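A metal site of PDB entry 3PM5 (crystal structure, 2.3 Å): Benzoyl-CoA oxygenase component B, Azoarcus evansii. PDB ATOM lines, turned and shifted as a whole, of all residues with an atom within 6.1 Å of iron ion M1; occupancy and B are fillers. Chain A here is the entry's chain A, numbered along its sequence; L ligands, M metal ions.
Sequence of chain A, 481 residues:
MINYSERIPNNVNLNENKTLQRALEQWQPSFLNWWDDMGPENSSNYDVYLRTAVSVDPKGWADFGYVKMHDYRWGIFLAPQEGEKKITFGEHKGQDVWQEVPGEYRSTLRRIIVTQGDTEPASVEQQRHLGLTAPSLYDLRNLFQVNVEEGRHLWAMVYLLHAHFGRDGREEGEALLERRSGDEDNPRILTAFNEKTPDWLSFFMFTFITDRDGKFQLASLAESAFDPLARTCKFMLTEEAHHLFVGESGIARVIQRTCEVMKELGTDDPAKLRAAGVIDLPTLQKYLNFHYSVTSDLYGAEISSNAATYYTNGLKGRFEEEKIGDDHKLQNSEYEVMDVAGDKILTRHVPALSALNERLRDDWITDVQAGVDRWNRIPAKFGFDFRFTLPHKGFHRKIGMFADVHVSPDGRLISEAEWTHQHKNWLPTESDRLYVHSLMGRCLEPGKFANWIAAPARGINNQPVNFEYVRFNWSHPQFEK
The side-chain carboxylate (OE2) of Glu 240 binds iron ion M1 (1.8 Å).
Iron ion M1 is bound by the side-chain carboxylate (OD2) of Asp 211.
ND1 of His 243 is bound to iron ion M1 (2.3 Å).
Iron ion M1 has three donor atoms within binding distance.
Three residues have an atom within 4 Å of iron ion M1: Asp 211, Glu 240 and His 243.
The nearest printed residue that does not touch iron ion M1 is Glu 150 (4.7 Å).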
ATOM      1  N   GLU A 120     -16.810  28.741  33.442  1.00  0.00           N
ATOM      2  CA  GLU A 120     -16.456  30.143  33.245  1.00  0.00           C
ATOM      3  C   GLU A 120     -15.219  30.527  34.065  1.00  0.00           C
ATOM      4  O   GLU A 120     -14.209  30.858  33.460  1.00  0.00           O
ATOM      5  CB  GLU A 120     -17.644  31.064  33.556  1.00  0.00           C
ATOM      6  CG  GLU A 120     -18.961  30.712  32.843  1.00  0.00           C
ATOM      7  CD  GLU A 120     -18.920  30.856  31.342  1.00  0.00           C
ATOM      8  OE1 GLU A 120     -17.948  31.539  30.845  1.00  0.00           O
ATOM      9  OE2 GLU A 120     -19.836  30.290  30.648  1.00  0.00           O
ATOM     10  N   VAL A 146     -11.853  38.371  26.731  1.00  0.00           N
ATOM     11  CA  VAL A 146     -12.451  37.083  26.798  1.00  0.00           C
ATOM     12  C   VAL A 146     -12.512  36.785  28.261  1.00  0.00           C
ATOM     13  O   VAL A 146     -13.546  36.370  28.745  1.00  0.00           O
ATOM     14  CB  VAL A 146     -11.615  36.028  25.943  1.00  0.00           C
ATOM     15  CG1 VAL A 146     -11.921  34.618  26.297  1.00  0.00           C
ATOM     16  CG2 VAL A 146     -11.785  36.228  24.412  1.00  0.00           C
ATOM     17  N   GLU A 150     -15.839  36.017  30.426  1.00  0.00           N
ATOM     18  CA  GLU A 150     -15.902  34.728  31.143  1.00  0.00           C
ATOM     19  C   GLU A 150     -16.406  35.051  32.555  1.00  0.00           C
ATOM     20  O   GLU A 150     -17.375  34.443  33.051  1.00  0.00           O
ATOM     21  CB  GLU A 150     -14.508  33.999  31.177  1.00  0.00           C
ATOM     22  CG  GLU A 150     -14.046  33.414  29.781  1.00  0.00           C
ATOM     23  CD  GLU A 150     -12.518  32.960  29.606  1.00  0.00           C
ATOM     24  OE1 GLU A 150     -11.561  33.454  30.236  1.00  0.00           O
ATOM     25  OE2 GLU A 150     -12.273  32.068  28.762  1.00  0.00           O
ATOM     26  N   HIS A 153     -19.992  35.887  32.785  1.00  0.00           N
ATOM     27  CA  HIS A 153     -20.808  34.697  32.632  1.00  0.00           C
ATOM     28  C   HIS A 153     -20.910  33.910  33.915  1.00  0.00           C
ATOM     29  O   HIS A 153     -21.947  33.328  34.187  1.00  0.00           O
ATOM     30  CB  HIS A 153     -20.235  33.872  31.500  1.00  0.00           C
ATOM     31  CG  HIS A 153     -20.445  34.515  30.175  1.00  0.00           C
ATOM     32  ND1 HIS A 153     -20.091  33.909  28.996  1.00  0.00           N
ATOM     33  CD2 HIS A 153     -21.039  35.683  29.845  1.00  0.00           C
ATOM     34  CE1 HIS A 153     -20.464  34.675  27.984  1.00  0.00           C
ATOM     35  NE2 HIS A 153     -21.033  35.760  28.479  1.00  0.00           N
ATOM     36  N   THR A 207     -10.589  28.829  22.004  1.00  0.00           N
ATOM     37  CA  THR A 207     -11.684  29.756  21.686  1.00  0.00           C
ATOM     38  C   THR A 207     -12.382  29.467  20.374  1.00  0.00           C
ATOM     39  O   THR A 207     -13.546  29.844  20.175  1.00  0.00           O
ATOM     40  CB  THR A 207     -11.271  31.198  21.767  1.00  0.00           C
ATOM     41  OG1 THR A 207     -10.092  31.395  20.988  1.00  0.00           O
ATOM     42  CG2 THR A 207     -10.983  31.544  23.231  1.00  0.00           C
ATOM     43  N   ASP A 211     -14.995  27.176  23.280  1.00  0.00           N
ATOM     44  CA  ASP A 211     -16.058  28.227  23.373  1.00  0.00           C
ATOM     45  C   ASP A 211     -17.252  27.904  22.502  1.00  0.00           C
ATOM     46  O   ASP A 211     -18.361  28.340  22.806  1.00  0.00           O
ATOM     47  CB  ASP A 211     -15.592  29.651  23.000  1.00  0.00           C
ATOM     48  CG  ASP A 211     -14.749  30.296  24.080  1.00  0.00           C
ATOM     49  OD1 ASP A 211     -13.817  29.646  24.541  1.00  0.00           O
ATOM     50  OD2 ASP A 211     -14.965  31.465  24.477  1.00  0.00           O
ATOM     51  N   GLU A 240     -20.566  35.811  23.338  1.00  0.00           N
ATOM     52  CA  GLU A 240     -19.708  34.693  22.885  1.00  0.00           C
ATOM     53  C   GLU A 240     -19.287  34.752  21.387  1.00  0.00           C
ATOM     54  O   GLU A 240     -18.259  34.195  21.028  1.00  0.00           O
ATOM     55  CB  GLU A 240     -20.359  33.338  23.213  1.00  0.00           C
ATOM     56  CG  GLU A 240     -19.409  32.149  23.226  1.00  0.00           C
ATOM     57  CD  GLU A 240     -18.605  32.019  24.551  1.00  0.00           C
ATOM     58  OE1 GLU A 240     -18.923  31.166  25.453  1.00  0.00           O
ATOM     59  OE2 GLU A 240     -17.618  32.765  24.681  1.00  0.00           O
ATOM     60  N   HIS A 243     -15.894  35.855  21.040  1.00  0.00           N
ATOM     61  CA  HIS A 243     -14.901  34.885  21.488  1.00  0.00           C
ATOM     62  C   HIS A 243     -14.567  33.935  20.357  1.00  0.00           C
ATOM     63  O   HIS A 243     -13.414  33.663  20.141  1.00  0.00           O
ATOM     64  CB  HIS A 243     -15.342  34.131  22.740  1.00  0.00           C
ATOM     65  CG  HIS A 243     -15.686  35.039  23.883  1.00  0.00           C
ATOM     66  ND1 HIS A 243     -15.936  34.583  25.147  1.00  0.00           N
ATOM     67  CD2 HIS A 243     -15.747  36.393  23.962  1.00  0.00           C
ATOM     68  CE1 HIS A 243     -16.192  35.598  25.944  1.00  0.00           C
ATOM     69  NE2 HIS A 243     -16.068  36.718  25.253  1.00  0.00           N
HETATM   70  N1  LIG L   1     -18.583  11.214  32.362  1.00  0.00           N
HETATM   71  O1  LIG L   1     -26.038  12.928  29.081  1.00  0.00           O
HETATM   72  P1  LIG L   1     -24.802  12.250  29.740  1.00  0.00           P
HETATM   73  C1  LIG L   1     -18.757  26.926  27.943  1.00  0.00           C
HETATM   74  C2  LIG L   1     -23.080   8.147  31.925  1.00  0.00           C
HETATM   75  S1  LIG L   1     -18.680  25.143  27.654  1.00  0.00           S
HETATM   76  C3  LIG L   1     -19.930  11.687  32.214  1.00  0.00           C
HETATM   77  O2  LIG L   1     -23.627  11.831  28.867  1.00  0.00           O
HETATM   78  P2  LIG L   1     -25.103  14.298  31.552  1.00  0.00           P
HETATM   79  C4  LIG L   1     -17.429  27.586  27.994  1.00  0.00           C
HETATM   80  C5  LIG L   1     -23.928   9.104  32.746  1.00  0.00           C
HETATM   81  O3  LIG L   1     -23.785   9.104  34.137  1.00  0.00           O
HETATM   82  C6  LIG L   1     -20.345  24.423  27.922  1.00  0.00           C
HETATM   83  N2  LIG L   1     -21.034  10.751  32.121  1.00  0.00           N
HETATM   84  O4  LIG L   1     -24.220  13.139  30.933  1.00  0.00           O
HETATM   85  C7  LIG L   1     -16.409  27.138  27.041  1.00  0.00           C
HETATM   86  C8  LIG L   1     -25.244   8.674  32.285  1.00  0.00           C
HETATM   87  O5  LIG L   1     -25.453   7.354  32.798  1.00  0.00           O
HETATM   88  P3  LIG L   1     -26.864   6.613  32.763  1.00  0.00           P
HETATM   89  C9  LIG L   1     -20.653  24.165  29.370  1.00  0.00           C
HETATM   90  C10 LIG L   1     -20.779   9.314  32.143  1.00  0.00           C
HETATM   91  O6  LIG L   1     -26.542  13.875  31.874  1.00  0.00           O
HETATM   92  C11 LIG L   1     -15.094  27.797  27.061  1.00  0.00           C
HETATM   93  C12 LIG L   1     -25.021   8.616  30.816  1.00  0.00           C
HETATM   94  O7  LIG L   1     -23.636   8.321  30.610  1.00  0.00           O
HETATM   95  N3  LIG L   1     -22.096  24.105  29.431  1.00  0.00           N
HETATM   96  O8  LIG L   1     -19.702  27.454  28.464  1.00  0.00           O
HETATM   97  O9  LIG L   1     -24.382  14.738  32.809  1.00  0.00           O
HETATM   98  C13 LIG L   1     -14.794  28.883  28.030  1.00  0.00           C
HETATM   99  C14 LIG L   1     -25.395   9.729  29.861  1.00  0.00           C
HETATM  100  O10 LIG L   1     -25.227  10.952  30.523  1.00  0.00           O
HETATM  101  C15 LIG L   1     -19.465   8.835  32.263  1.00  0.00           C
HETATM  102  C16 LIG L   1     -22.754  22.886  29.678  1.00  0.00           C
HETATM  103  O11 LIG L   1     -22.104  21.864  29.870  1.00  0.00           O
HETATM  104  C17 LIG L   1     -18.335   9.805  32.376  1.00  0.00           C
HETATM  105  N4  LIG L   1     -17.036   9.300  32.493  1.00  0.00           N
HETATM  106  O12 LIG L   1     -25.147  15.479  30.431  1.00  0.00           O
HETATM  107  C18 LIG L   1     -15.829  29.308  28.989  1.00  0.00           C
HETATM  108  C19 LIG L   1     -24.301  22.923  29.641  1.00  0.00           C
HETATM  109  N5  LIG L   1     -19.492   7.490  32.257  1.00  0.00           N
HETATM  110  O13 LIG L   1     -27.738   7.274  33.806  1.00  0.00           O
HETATM  111  C20 LIG L   1     -17.158  28.666  28.965  1.00  0.00           C
HETATM  112  C21 LIG L   1     -25.063  22.175  30.671  1.00  0.00           C
HETATM  113  C22 LIG L   1     -20.791   7.084  32.132  1.00  0.00           C
HETATM  114  O14 LIG L   1     -26.642   5.157  33.051  1.00  0.00           O
HETATM  115  N6  LIG L   1     -24.719  20.777  30.752  1.00  0.00           N
HETATM  116  N7  LIG L   1     -21.587   8.215  32.079  1.00  0.00           N
HETATM  117  O15 LIG L   1     -27.533   6.804  31.384  1.00  0.00           O
HETATM  118  C23 LIG L   1     -25.483  19.695  30.213  1.00  0.00           C
HETATM  119  O16 LIG L   1     -26.562  19.840  29.610  1.00  0.00           O
HETATM  120  C24 LIG L   1     -24.838  18.381  30.511  1.00  0.00           C
HETATM  121  O17 LIG L   1     -23.748  18.715  31.287  1.00  0.00           O
HETATM  122  C25 LIG L   1     -24.308  17.542  29.331  1.00  0.00           C
HETATM  123  C26 LIG L   1     -23.971  16.103  29.882  1.00  0.00           C
HETATM  124  C27 LIG L   1     -25.296  17.440  28.224  1.00  0.00           C
HETATM  125  C28 LIG L   1     -23.029  18.177  28.807  1.00  0.00           C
HETATM  126 FE    FE M   1     -16.185  32.398  25.775  1.00  0.00          FE
HETATM  127 FE    FE M   2     -18.727  31.937  28.473  1.00  0.00          FE
